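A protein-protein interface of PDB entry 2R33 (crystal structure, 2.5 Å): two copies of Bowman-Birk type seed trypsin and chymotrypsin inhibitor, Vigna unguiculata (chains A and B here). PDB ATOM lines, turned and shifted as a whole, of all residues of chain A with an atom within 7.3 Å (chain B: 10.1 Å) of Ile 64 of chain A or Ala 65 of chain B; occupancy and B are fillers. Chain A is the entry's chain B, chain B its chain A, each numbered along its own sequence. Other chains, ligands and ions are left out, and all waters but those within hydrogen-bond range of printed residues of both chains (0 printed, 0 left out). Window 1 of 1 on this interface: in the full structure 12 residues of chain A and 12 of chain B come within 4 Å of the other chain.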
ATOM      1  N   VAL A  23      -4.387  10.660  18.410  1.00  0.00           N
ATOM      2  CA  VAL A  23      -5.462  11.440  18.989  1.00  0.00           C
ATOM      3  C   VAL A  23      -6.421  11.909  17.892  1.00  0.00           C
ATOM      4  O   VAL A  23      -5.969  12.527  16.929  1.00  0.00           O
ATOM      5  CB  VAL A  23      -4.952  12.681  19.756  1.00  0.00           C
ATOM      6  CG1 VAL A  23      -6.126  13.414  20.391  1.00  0.00           C
ATOM      7  CG2 VAL A  23      -3.912  12.317  20.810  1.00  0.00           C
ATOM      8  N   THR A  25     -10.281  13.888  16.893  1.00  0.00           N
ATOM      9  CA  THR A  25     -11.292  14.814  17.409  1.00  0.00           C
ATOM     10  C   THR A  25     -12.612  14.074  17.617  1.00  0.00           C
ATOM     11  O   THR A  25     -12.807  13.022  17.004  1.00  0.00           O
ATOM     12  CB  THR A  25     -11.515  15.982  16.443  1.00  0.00           C
ATOM     13  OG1 THR A  25     -12.011  15.432  15.204  1.00  0.00           O
ATOM     14  CG2 THR A  25     -10.237  16.764  16.203  1.00  0.00           C
ATOM     15  N   PRO A  30     -14.097  12.132  11.479  1.00  0.00           N
ATOM     16  CA  PRO A  30     -13.048  12.022  12.475  1.00  0.00           C
ATOM     17  C   PRO A  30     -11.738  12.584  11.945  1.00  0.00           C
ATOM     18  O   PRO A  30     -11.332  12.380  10.801  1.00  0.00           O
ATOM     19  CB  PRO A  30     -12.961  10.532  12.773  1.00  0.00           C
ATOM     20  CG  PRO A  30     -13.612   9.842  11.627  1.00  0.00           C
ATOM     21  CD  PRO A  30     -14.564  10.815  10.993  1.00  0.00           C
ATOM     22  N   GLN A  31     -11.059  13.367  12.777  1.00  0.00           N
ATOM     23  CA  GLN A  31      -9.768  13.956  12.430  1.00  0.00           C
ATOM     24  C   GLN A  31      -8.736  13.427  13.419  1.00  0.00           C
ATOM     25  O   GLN A  31      -8.914  13.571  14.636  1.00  0.00           O
ATOM     26  CB  GLN A  31      -9.859  15.473  12.386  1.00  0.00           C
ATOM     27  CG  GLN A  31     -10.774  15.973  11.270  1.00  0.00           C
ATOM     28  CD  GLN A  31     -10.135  15.833   9.898  1.00  0.00           C
ATOM     29  OE1 GLN A  31     -10.207  14.764   9.269  1.00  0.00           O
ATOM     30  NE2 GLN A  31      -9.496  16.908   9.466  1.00  0.00           N
ATOM     31  N   CYS A  32      -7.734  12.716  12.939  1.00  0.00           N
ATOM     32  CA  CYS A  32      -6.766  12.077  13.811  1.00  0.00           C
ATOM     33  C   CYS A  32      -5.339  12.410  13.399  1.00  0.00           C
ATOM     34  O   CYS A  32      -5.049  12.431  12.205  1.00  0.00           O
ATOM     35  CB  CYS A  32      -6.912  10.548  13.729  1.00  0.00           C
ATOM     36  SG  CYS A  32      -8.581   9.885  13.834  1.00  0.00           S
ATOM     37  N   HIS A  33      -4.445  12.462  14.384  1.00  0.00           N
ATOM     38  CA  HIS A  33      -3.044  12.703  14.063  1.00  0.00           C
ATOM     39  C   HIS A  33      -2.163  11.978  15.073  1.00  0.00           C
ATOM     40  O   HIS A  33      -2.620  11.584  16.153  1.00  0.00           O
ATOM     41  CB  HIS A  33      -2.706  14.198  14.029  1.00  0.00           C
ATOM     42  CG  HIS A  33      -2.929  14.827  15.366  1.00  0.00           C
ATOM     43  ND1 HIS A  33      -4.201  14.911  15.895  1.00  0.00           N
ATOM     44  CD2 HIS A  33      -2.086  15.375  16.270  1.00  0.00           C
ATOM     45  CE1 HIS A  33      -4.131  15.489  17.089  1.00  0.00           C
ATOM     46  NE2 HIS A  33      -2.858  15.787  17.338  1.00  0.00           N
ATOM     47  N   CYS A  34      -0.938  11.696  14.627  1.00  0.00           N
ATOM     48  CA  CYS A  34      -0.012  11.017  15.524  1.00  0.00           C
ATOM     49  C   CYS A  34       0.882  12.027  16.245  1.00  0.00           C
ATOM     50  O   CYS A  34       1.617  12.807  15.648  1.00  0.00           O
ATOM     51  CB  CYS A  34       0.825  10.025  14.717  1.00  0.00           C
ATOM     52  SG  CYS A  34       1.798   8.911  15.743  1.00  0.00           S
ATOM     53  N   CYS A  61       4.952  13.978  13.147  1.00  0.00           N
ATOM     54  CA  CYS A  61       4.249  13.988  11.859  1.00  0.00           C
ATOM     55  C   CYS A  61       3.024  14.899  11.993  1.00  0.00           C
ATOM     56  O   CYS A  61       2.268  14.741  12.955  1.00  0.00           O
ATOM     57  CB  CYS A  61       3.887  12.583  11.420  1.00  0.00           C
ATOM     58  SG  CYS A  61       3.286  12.392   9.724  1.00  0.00           S
ATOM     59  N   LEU A  62       2.864  15.872  11.107  1.00  0.00           N
ATOM     60  CA  LEU A  62       1.712  16.756  11.139  1.00  0.00           C
ATOM     61  C   LEU A  62       0.526  16.171  10.379  1.00  0.00           C
ATOM     62  O   LEU A  62      -0.595  16.612  10.596  1.00  0.00           O
ATOM     63  CB  LEU A  62       2.010  18.160  10.583  1.00  0.00           C
ATOM     64  CG  LEU A  62       3.361  18.738  11.048  1.00  0.00           C
ATOM     65  CD1 LEU A  62       3.783  19.913  10.187  1.00  0.00           C
ATOM     66  CD2 LEU A  62       3.339  19.144  12.517  1.00  0.00           C
ATOM     67  N   ASP A  63       0.726  15.190   9.513  1.00  0.00           N
ATOM     68  CA  ASP A  63      -0.348  14.568   8.766  1.00  0.00           C
ATOM     69  C   ASP A  63      -1.644  14.361   9.547  1.00  0.00           C
ATOM     70  O   ASP A  63      -1.703  13.784  10.632  1.00  0.00           O
ATOM     71  CB  ASP A  63       0.140  13.220   8.214  1.00  0.00           C
ATOM     72  CG  ASP A  63       1.230  13.343   7.175  1.00  0.00           C
ATOM     73  OD1 ASP A  63       1.595  14.432   6.698  1.00  0.00           O
ATOM     74  OD2 ASP A  63       1.798  12.296   6.800  1.00  0.00           O
ATOM     75  N   ILE A  64      -2.772  14.802   9.006  1.00  0.00           N
ATOM     76  CA  ILE A  64      -4.081  14.520   9.584  1.00  0.00           C
ATOM     77  C   ILE A  64      -4.848  13.557   8.675  1.00  0.00           C
ATOM     78  O   ILE A  64      -4.945  13.685   7.437  1.00  0.00           O
ATOM     79  CB  ILE A  64      -4.883  15.798   9.833  1.00  0.00           C
ATOM     80  CG1 ILE A  64      -4.102  16.763  10.749  1.00  0.00           C
ATOM     81  CG2 ILE A  64      -6.240  15.498  10.452  1.00  0.00           C
ATOM     82  CD1 ILE A  64      -4.495  18.215  10.549  1.00  0.00           C
ATOM     83  N   ALA A  65      -5.334  12.477   9.302  1.00  0.00           N
ATOM     84  CA  ALA A  65      -6.076  11.469   8.533  1.00  0.00           C
ATOM     85  C   ALA A  65      -7.446  11.246   9.156  1.00  0.00           C
ATOM     86  O   ALA A  65      -7.731  11.772  10.234  1.00  0.00           O
ATOM     87  CB  ALA A  65      -5.279  10.187   8.416  1.00  0.00           C
ATOM     88  N   ASN A  66      -8.269  10.409   8.500  1.00  0.00           N
ATOM     89  CA  ASN A  66      -9.601  10.150   9.054  1.00  0.00           C
ATOM     90  C   ASN A  66      -9.581   8.960   9.994  1.00  0.00           C
ATOM     91  O   ASN A  66     -10.591   8.599  10.598  1.00  0.00           O
ATOM     92  CB  ASN A  66     -10.632  10.037   7.944  1.00  0.00           C
ATOM     93  CG  ASN A  66     -11.100  11.370   7.395  1.00  0.00           C
ATOM     94  OD1 ASN A  66     -12.161  11.438   6.760  1.00  0.00           O
ATOM     95  ND2 ASN A  66     -10.403  12.477   7.566  1.00  0.00           N
ATOM     96  N   PHE A  67      -8.389   8.401  10.203  1.00  0.00           N
ATOM     97  CA  PHE A  67      -8.177   7.206  10.998  1.00  0.00           C
ATOM     98  C   PHE A  67      -6.776   7.194  11.610  1.00  0.00           C
ATOM     99  O   PHE A  67      -5.935   8.041  11.329  1.00  0.00           O
ATOM    100  CB  PHE A  67      -8.294   5.958  10.083  1.00  0.00           C
ATOM    101  CG  PHE A  67      -7.278   6.051   8.974  1.00  0.00           C
ATOM    102  CD1 PHE A  67      -7.545   6.789   7.837  1.00  0.00           C
ATOM    103  CD2 PHE A  67      -6.038   5.444   9.099  1.00  0.00           C
ATOM    104  CE1 PHE A  67      -6.602   6.912   6.838  1.00  0.00           C
ATOM    105  CE2 PHE A  67      -5.074   5.586   8.120  1.00  0.00           C
ATOM    106  CZ  PHE A  67      -5.376   6.310   6.991  1.00  0.00           C
ATOM    107  N   CYS B  22      -5.190  11.683  -6.909  1.00  0.00           N
ATOM    108  CA  CYS B  22      -5.706  12.019  -5.599  1.00  0.00           C
ATOM    109  C   CYS B  22      -6.864  12.992  -5.726  1.00  0.00           C
ATOM    110  O   CYS B  22      -6.697  14.073  -6.291  1.00  0.00           O
ATOM    111  CB  CYS B  22      -4.557  12.589  -4.757  1.00  0.00           C
ATOM    112  SG  CYS B  22      -4.936  12.785  -2.994  1.00  0.00           S
ATOM    113  N   VAL B  23      -8.041  12.601  -5.272  1.00  0.00           N
ATOM    114  CA  VAL B  23      -9.212  13.469  -5.369  1.00  0.00           C
ATOM    115  C   VAL B  23      -9.556  13.966  -3.971  1.00  0.00           C
ATOM    116  O   VAL B  23      -9.933  13.196  -3.083  1.00  0.00           O
ATOM    117  CB  VAL B  23     -10.397  12.730  -6.015  1.00  0.00           C
ATOM    118  CG1 VAL B  23     -11.668  13.561  -6.062  1.00  0.00           C
ATOM    119  CG2 VAL B  23      -9.988  12.258  -7.417  1.00  0.00           C
ATOM    120  N   CYS B  24      -9.349  15.265  -3.769  1.00  0.00           N
ATOM    121  CA  CYS B  24      -9.687  15.892  -2.511  1.00  0.00           C
ATOM    122  C   CYS B  24     -10.828  16.846  -2.667  1.00  0.00           C
ATOM    123  O   CYS B  24     -10.923  17.580  -3.642  1.00  0.00           O
ATOM    124  CB  CYS B  24      -8.527  16.694  -1.927  1.00  0.00           C
ATOM    125  SG  CYS B  24      -6.888  16.216  -2.560  1.00  0.00           S
ATOM    126  N   THR B  25     -11.650  16.807  -1.630  1.00  0.00           N
ATOM    127  CA  THR B  25     -12.767  17.719  -1.536  1.00  0.00           C
ATOM    128  C   THR B  25     -12.313  19.043  -0.970  1.00  0.00           C
ATOM    129  O   THR B  25     -11.430  19.149  -0.110  1.00  0.00           O
ATOM    130  CB  THR B  25     -13.872  17.201  -0.640  1.00  0.00           C
ATOM    131  OG1 THR B  25     -13.380  17.152   0.698  1.00  0.00           O
ATOM    132  CG2 THR B  25     -14.339  15.821  -1.091  1.00  0.00           C
ATOM    133  N   LYS B  26     -13.005  20.073  -1.541  1.00  0.00           N
ATOM    134  CA  LYS B  26     -12.920  21.531  -1.378  1.00  0.00           C
ATOM    135  C   LYS B  26     -13.442  22.083  -0.043  1.00  0.00           C
ATOM    136  O   LYS B  26     -13.803  23.254   0.071  1.00  0.00           O
ATOM    137  CB  LYS B  26     -13.746  22.159  -2.496  1.00  0.00           C
ATOM    138  CG  LYS B  26     -15.151  21.590  -2.614  1.00  0.00           C
ATOM    139  CD  LYS B  26     -15.099  20.073  -2.683  1.00  0.00           C
ATOM    140  CE  LYS B  26     -16.471  19.457  -2.881  1.00  0.00           C
ATOM    141  NZ  LYS B  26     -16.448  17.980  -2.707  1.00  0.00           N
ATOM    142  N   SER B  27     -13.364  21.156   0.954  1.00  0.00           N
ATOM    143  CA  SER B  27     -14.091  21.540   2.179  1.00  0.00           C
ATOM    144  C   SER B  27     -13.078  21.941   3.166  1.00  0.00           C
ATOM    145  O   SER B  27     -11.841  21.921   2.895  1.00  0.00           O
ATOM    146  CB  SER B  27     -14.722  20.138   2.626  1.00  0.00           C
ATOM    147  OG  SER B  27     -14.560  19.153   2.000  1.00  0.00           O
ATOM    148  N   ILE B  28     -13.429  22.312   4.444  1.00  0.00           N
ATOM    149  CA  ILE B  28     -12.521  22.495   5.560  1.00  0.00           C
ATOM    150  C   ILE B  28     -13.118  21.649   6.688  1.00  0.00           C
ATOM    151  O   ILE B  28     -14.229  21.938   7.125  1.00  0.00           O
ATOM    152  CB  ILE B  28     -12.373  23.935   6.033  1.00  0.00           C
ATOM    153  CG1 ILE B  28     -11.798  24.860   4.954  1.00  0.00           C
ATOM    154  CG2 ILE B  28     -11.507  24.011   7.290  1.00  0.00           C
ATOM    155  CD1 ILE B  28     -12.181  26.317   5.199  1.00  0.00           C
ATOM    156  N   PRO B  29     -12.478  20.552   7.039  1.00  0.00           N
ATOM    157  CA  PRO B  29     -11.188  20.190   6.503  1.00  0.00           C
ATOM    158  C   PRO B  29     -11.274  19.411   5.210  1.00  0.00           C
ATOM    159  O   PRO B  29     -12.334  18.908   4.861  1.00  0.00           O
ATOM    160  CB  PRO B  29     -10.606  19.254   7.581  1.00  0.00           C
ATOM    161  CG  PRO B  29     -11.820  18.558   8.099  1.00  0.00           C
ATOM    162  CD  PRO B  29     -12.901  19.616   8.113  1.00  0.00           C
ATOM    163  N   PRO B  30     -10.196  19.448   4.437  1.00  0.00           N
ATOM    164  CA  PRO B  30     -10.135  18.726   3.190  1.00  0.00           C
ATOM    165  C   PRO B  30     -10.303  17.222   3.396  1.00  0.00           C
ATOM    166  O   PRO B  30      -9.879  16.670   4.418  1.00  0.00           O
ATOM    167  CB  PRO B  30      -8.743  19.015   2.639  1.00  0.00           C
ATOM    168  CG  PRO B  30      -8.009  19.777   3.674  1.00  0.00           C
ATOM    169  CD  PRO B  30      -8.917  20.095   4.807  1.00  0.00           C
ATOM    170  N   GLN B  31     -10.935  16.558   2.433  1.00  0.00           N
ATOM    171  CA  GLN B  31     -11.108  15.114   2.449  1.00  0.00           C
ATOM    172  C   GLN B  31     -10.542  14.533   1.141  1.00  0.00           C
ATOM    173  O   GLN B  31     -11.104  14.719   0.061  1.00  0.00           O
ATOM    174  CB  GLN B  31     -12.529  14.641   2.700  1.00  0.00           C
ATOM    175  CG  GLN B  31     -13.040  15.050   4.076  1.00  0.00           C
ATOM    176  CD  GLN B  31     -12.510  14.179   5.187  1.00  0.00           C
ATOM    177  OE1 GLN B  31     -11.385  14.293   5.662  1.00  0.00           O
ATOM    178  NE2 GLN B  31     -13.372  13.274   5.614  1.00  0.00           N
ATOM    179  N   CYS B  32      -9.407  13.860   1.272  1.00  0.00           N
ATOM    180  CA  CYS B  32      -8.696  13.279   0.150  1.00  0.00           C
ATOM    181  C   CYS B  32      -8.700  11.749   0.111  1.00  0.00           C
ATOM    182  O   CYS B  32      -8.751  11.041   1.120  1.00  0.00           O
ATOM    183  CB  CYS B  32      -7.228  13.747   0.159  1.00  0.00           C
ATOM    184  SG  CYS B  32      -6.987  15.536   0.191  1.00  0.00           S
ATOM    185  N   HIS B  33      -8.556  11.206  -1.108  1.00  0.00           N
ATOM    186  CA  HIS B  33      -8.470   9.748  -1.241  1.00  0.00           C
ATOM    187  C   HIS B  33      -7.783   9.388  -2.539  1.00  0.00           C
ATOM    188  O   HIS B  33      -7.768  10.194  -3.452  1.00  0.00           O
ATOM    189  CB  HIS B  33      -9.816   9.032  -1.096  1.00  0.00           C
ATOM    190  CG  HIS B  33     -10.753   9.280  -2.223  1.00  0.00           C
ATOM    191  ND1 HIS B  33     -11.554  10.395  -2.311  1.00  0.00           N
ATOM    192  CD2 HIS B  33     -11.014   8.556  -3.336  1.00  0.00           C
ATOM    193  CE1 HIS B  33     -12.268  10.351  -3.426  1.00  0.00           C
ATOM    194  NE2 HIS B  33     -11.965   9.244  -4.069  1.00  0.00           N
ATOM    195  N   CYS B  34      -7.096   8.265  -2.563  1.00  0.00           N
ATOM    196  CA  CYS B  34      -6.399   7.827  -3.771  1.00  0.00           C
ATOM    197  C   CYS B  34      -7.318   6.931  -4.599  1.00  0.00           C
ATOM    198  O   CYS B  34      -7.941   6.030  -4.036  1.00  0.00           O
ATOM    199  CB  CYS B  34      -5.096   7.125  -3.400  1.00  0.00           C
ATOM    200  SG  CYS B  34      -3.957   6.919  -4.798  1.00  0.00           S
ATOM    201  N   HIS B  43      -0.834   0.559  -1.939  1.00  0.00           N
ATOM    202  CA  HIS B  43       0.512   1.049  -1.644  1.00  0.00           C
ATOM    203  C   HIS B  43       0.872   0.696  -0.206  1.00  0.00           C
ATOM    204  O   HIS B  43       0.046   0.089   0.481  1.00  0.00           O
ATOM    205  CB  HIS B  43       0.673   2.541  -1.905  1.00  0.00           C
ATOM    206  CG  HIS B  43      -0.452   3.379  -1.400  1.00  0.00           C
ATOM    207  ND1 HIS B  43      -1.552   3.615  -2.189  1.00  0.00           N
ATOM    208  CD2 HIS B  43      -0.684   4.023  -0.226  1.00  0.00           C
ATOM    209  CE1 HIS B  43      -2.414   4.371  -1.520  1.00  0.00           C
ATOM    210  NE2 HIS B  43      -1.909   4.636  -0.323  1.00  0.00           N
ATOM    211  N   GLY B  45       1.355   2.631   2.547  1.00  0.00           N
ATOM    212  CA  GLY B  45       0.760   3.319   3.706  1.00  0.00           C
ATOM    213  C   GLY B  45      -0.733   3.065   3.875  1.00  0.00           C
ATOM    214  O   GLY B  45      -1.380   3.672   4.720  1.00  0.00           O
ATOM    215  N   CYS B  46      -1.307   2.170   3.095  1.00  0.00           N
ATOM    216  CA  CYS B  46      -2.718   1.888   3.107  1.00  0.00           C
ATOM    217  C   CYS B  46      -3.225   0.994   4.228  1.00  0.00           C
ATOM    218  O   CYS B  46      -2.913  -0.187   4.360  1.00  0.00           O
ATOM    219  CB  CYS B  46      -3.134   1.274   1.753  1.00  0.00           C
ATOM    220  SG  CYS B  46      -4.944   1.218   1.683  1.00  0.00           S
ATOM    221  N   LYS B  47      -4.115   1.589   5.012  1.00  0.00           N
ATOM    222  CA  LYS B  47      -4.801   0.928   6.112  1.00  0.00           C
ATOM    223  C   LYS B  47      -5.900   0.024   5.570  1.00  0.00           C
ATOM    224  O   LYS B  47      -5.961  -1.145   5.906  1.00  0.00           O
ATOM    225  CB  LYS B  47      -5.378   1.997   7.035  1.00  0.00           C
ATOM    226  CG  LYS B  47      -6.420   1.577   8.055  1.00  0.00           C
ATOM    227  CD  LYS B  47      -5.790   1.348   9.428  1.00  0.00           C
ATOM    228  CE  LYS B  47      -6.820   1.516  10.537  1.00  0.00           C
ATOM    229  NZ  LYS B  47      -6.340   0.887  11.800  1.00  0.00           N
ATOM    230  N   CYS B  61      -7.194   1.753  -2.486  1.00  0.00           N
ATOM    231  CA  CYS B  61      -7.123   2.153  -1.082  1.00  0.00           C
ATOM    232  C   CYS B  61      -8.315   3.025  -0.734  1.00  0.00           C
ATOM    233  O   CYS B  61      -8.580   4.015  -1.397  1.00  0.00           O
ATOM    234  CB  CYS B  61      -5.779   2.814  -0.771  1.00  0.00           C
ATOM    235  SG  CYS B  61      -5.406   3.083   0.983  1.00  0.00           S
ATOM    236  N   LEU B  62      -9.081   2.641   0.272  1.00  0.00           N
ATOM    237  CA  LEU B  62     -10.241   3.364   0.772  1.00  0.00           C
ATOM    238  C   LEU B  62      -9.898   4.427   1.804  1.00  0.00           C
ATOM    239  O   LEU B  62     -10.756   5.247   2.125  1.00  0.00           O
ATOM    240  CB  LEU B  62     -11.200   2.359   1.385  1.00  0.00           C
ATOM    241  CG  LEU B  62     -12.241   1.634   0.536  1.00  0.00           C
ATOM    242  CD1 LEU B  62     -11.996   1.654  -0.970  1.00  0.00           C
ATOM    243  CD2 LEU B  62     -12.388   0.197   1.034  1.00  0.00           C
ATOM    244  N   ASP B  63      -8.676   4.471   2.343  1.00  0.00           N
ATOM    245  CA  ASP B  63      -8.330   5.488   3.319  1.00  0.00           C
ATOM    246  C   ASP B  63      -8.724   6.895   2.871  1.00  0.00           C
ATOM    247  O   ASP B  63      -8.453   7.302   1.740  1.00  0.00           O
ATOM    248  CB  ASP B  63      -6.831   5.542   3.592  1.00  0.00           C
ATOM    249  CG  ASP B  63      -6.210   4.277   4.134  1.00  0.00           C
ATOM    250  OD1 ASP B  63      -6.950   3.291   4.379  1.00  0.00           O
ATOM    251  OD2 ASP B  63      -4.959   4.305   4.266  1.00  0.00           O
ATOM    252  N   ILE B  64      -9.263   7.685   3.791  1.00  0.00           N
ATOM    253  CA  ILE B  64      -9.543   9.092   3.569  1.00  0.00           C
ATOM    254  C   ILE B  64      -8.638   9.900   4.497  1.00  0.00           C
ATOM    255  O   ILE B  64      -8.561   9.619   5.697  1.00  0.00           O
ATOM    256  CB  ILE B  64     -10.994   9.486   3.806  1.00  0.00           C
ATOM    257  CG1 ILE B  64     -11.901   8.803   2.758  1.00  0.00           C
ATOM    258  CG2 ILE B  64     -11.218  10.986   3.719  1.00  0.00           C
ATOM    259  CD1 ILE B  64     -13.201   8.441   3.475  1.00  0.00           C
ATOM    260  N   ALA B  65      -7.931  10.863   3.930  1.00  0.00           N
ATOM    261  CA  ALA B  65      -7.050  11.712   4.724  1.00  0.00           C
ATOM    262  C   ALA B  65      -7.243  13.176   4.328  1.00  0.00           C
ATOM    263  O   ALA B  65      -8.061  13.501   3.471  1.00  0.00           O
ATOM    264  CB  ALA B  65      -5.625  11.213   4.574  1.00  0.00           C
ATOM    265  N   ASN B  66      -6.517  14.093   4.961  1.00  0.00           N
ATOM    266  CA  ASN B  66      -6.614  15.503   4.662  1.00  0.00           C
ATOM    267  C   ASN B  66      -5.607  15.934   3.613  1.00  0.00           C
ATOM    268  O   ASN B  66      -5.544  17.122   3.336  1.00  0.00           O
ATOM    269  CB  ASN B  66      -6.406  16.377   5.907  1.00  0.00           C
ATOM    270  CG  ASN B  66      -7.527  16.269   6.919  1.00  0.00           C
ATOM    271  OD1 ASN B  66      -7.582  17.097   7.831  1.00  0.00           O
ATOM    272  ND2 ASN B  66      -8.401  15.288   6.810  1.00  0.00           N
ATOM    273  N   PHE B  67      -4.811  15.031   3.076  1.00  0.00           N
ATOM    274  CA  PHE B  67      -3.743  15.392   2.152  1.00  0.00           C
ATOM    275  C   PHE B  67      -3.505  14.272   1.153  1.00  0.00           C
ATOM    276  O   PHE B  67      -4.001  13.162   1.337  1.00  0.00           O
ATOM    277  CB  PHE B  67      -2.440  15.642   2.954  1.00  0.00           C
ATOM    278  CG  PHE B  67      -2.004  14.358   3.620  1.00  0.00           C
ATOM    279  CD1 PHE B  67      -1.102  13.486   3.014  1.00  0.00           C
ATOM    280  CD2 PHE B  67      -2.582  13.986   4.821  1.00  0.00           C
ATOM    281  CE1 PHE B  67      -0.763  12.287   3.632  1.00  0.00           C
ATOM    282  CE2 PHE B  67      -2.244  12.801   5.440  1.00  0.00           C
ATOM    283  CZ  PHE B  67      -1.330  11.945   4.847  1.00  0.00           C
ATOM    284  N   CYS B  68      -2.611  14.502   0.209  1.00  0.00           N
ATOM    285  CA  CYS B  68      -2.247  13.541  -0.820  1.00  0.00           C
ATOM    286  C   CYS B  68      -0.797  13.096  -0.765  1.00  0.00           C
ATOM    287  O   CYS B  68       0.094  13.907  -0.528  1.00  0.00           O
ATOM    288  CB  CYS B  68      -2.450  14.210  -2.191  1.00  0.00           C
ATOM    289  SG  CYS B  68      -4.171  14.639  -2.600  1.00  0.00           S
ATOM    290  N   TYR B  69      -0.489  11.837  -1.027  1.00  0.00           N
ATOM    291  CA  TYR B  69       0.907  11.427  -1.155  1.00  0.00           C
ATOM    292  C   TYR B  69       1.421  11.953  -2.501  1.00  0.00           C
ATOM    293  O   TYR B  69       0.609  12.362  -3.332  1.00  0.00           O
ATOM    294  CB  TYR B  69       1.102   9.913  -1.089  1.00  0.00           C
ATOM    295  CG  TYR B  69       0.955   9.406   0.330  1.00  0.00           C
ATOM    296  CD1 TYR B  69       1.902   9.724   1.288  1.00  0.00           C
ATOM    297  CD2 TYR B  69      -0.114   8.612   0.707  1.00  0.00           C
ATOM    298  CE1 TYR B  69       1.778   9.285   2.595  1.00  0.00           C
ATOM    299  CE2 TYR B  69      -0.245   8.152   2.007  1.00  0.00           C
ATOM    300  CZ  TYR B  69       0.699   8.502   2.944  1.00  0.00           C
ATOM    301  OH  TYR B  69       0.577   8.062   4.240  1.00  0.00           O
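Among the printed residues, merely in contact across the chains: Gln 31 of chain A with Pro 29 of chain B (3.2 Å), Phe 67 of chain A with Asp 63 of chain B (3.4 Å), Ile 64 of chain A with Phe 67 of chain B (3.5 Å), Phe 67 of chain A with Ile 64 of chain B (3.5 Å), Asn 66 of chain A with Asn 66 of chain B (3.5 Å), Asp 63 of chain A with Phe 67 of chain B (3.7 Å), Phe 67 of chain A with Lys 47 of chain B (3.8 Å), Gln 31 of chain A with Gln 31 of chain B (3.8 Å), Ile 64 of chain A with Ala 65 of chain B (3.8 Å), Ala 65 of chain A with Ala 65 of chain B (3.9 Å) and Ala 65 of chain A with Ile 64 of chain B (3.98 Å).
Hydrophobic or aromatic side chains of chain A that line the printed part of chain B: Ile 64, Ala 65 and Phe 67.
Of the 26 printed residues of chain B, 8 touch a printed residue of chain A.
Among the printed residues, no Asp or Glu carboxylate lies within 4 Å of a Lys or Arg side-chain nitrogen of the other chain.
The backbone carbonyl oxygen of Gln 31 of chain A sits at hydrogen-bond distance from the backbone NH of Thr 25 of chain A (2.7 Å).
The side-chain sulfur (SG) of Cys 46 of chain B forms a disulfide with the side-chain sulfur (SG) of Cys 61 of chain B (2.0 Å).
N of Phe 67 of chain B is in hydrogen-bond range of SG of Cys 32 of chain B, 3.6 Å away.
The backbone carbonyl oxygen (O) of Pro 30 of chain A sits close to the side-chain amide nitrogen (ND2) of Asn 66 of chain A, at 3.4 Å.
The backbone NH (N) of Cys 32 of chain A is in hydrogen-bond range of the backbone carbonyl oxygen (O) of Ala 65 of chain A (2.9 Å).
The backbone NH of Lys 47 of chain B lies within hydrogen-bond range of the side-chain carboxylate of Asp 63 of chain B (2.9 Å).
Gln 31 of chain A touches its own counterpart, Gln 31 of chain B.
Ile 64 of chain A touches Ala 65 of chain B, and with the chains exchanged Ala 65 of chain A touches Ile 64 of chain B.
Ile 64 of chain A touches Phe 67 of chain B, and with the chains exchanged Phe 67 of chain A touches Ile 64 of chain B.
Ala 65 of chain A touches its own counterpart, Ala 65 of chain B.
Of the 15 pairs that touch across the chains among the printed residues, 13 have their exchanged pair printed and touching as well.
N of Asn 66 of chain B lies within hydrogen-bond range of O of Ile 64 of chain A, 3.0 Å away.
NE2 of Gln 31 of chain A lies within hydrogen-bond range of OD1 of Asn 66 of chain B, at 2.5 Å.
NE2 of Gln 31 of chain B sits at hydrogen-bond distance from OD1 of Asn 66 of chain A (2.5 Å).
The backbone NH (N) of Asn 66 of chain A sits at hydrogen-bond distance from the backbone carbonyl oxygen (O) of Ile 64 of chain B, at 2.9 Å.
Of chain B, only Pro 29, Gln 31 and Asn 66 come within 4 Å of Gln 31 of chain A.
Printed residues of chain B within 4 Å of Asp 63 of chain A: Phe 67 (3.7 Å).
Ile 64 of chain A touches just these residues of chain B: Ala 65 (3.8 Å), Asn 66 (3.0 Å) and Phe 67 (3.5 Å).
Of the printed residues of chain A, Pro 29 of chain B touches Gln 31.
Of the printed residues of chain A, Gln 31 of chain B touches Gln 31 (3.8 Å) and Asn 66 (2.5 Å).
Of the printed residues of chain A, Ala 65 of chain B touches Ile 64 and Ala 65.
Of the printed residues of chain A, Asn 66 of chain B touches Gln 31, Ile 64 and Asn 66.
The nearest residue of chain B that does not touch Ile 64 of chain A is Ile 64 of chain B (5.7 Å).
The nearest residue of chain A that does not touch Ala 65 of chain B is Asn 66 of chain A (4.2 Å).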
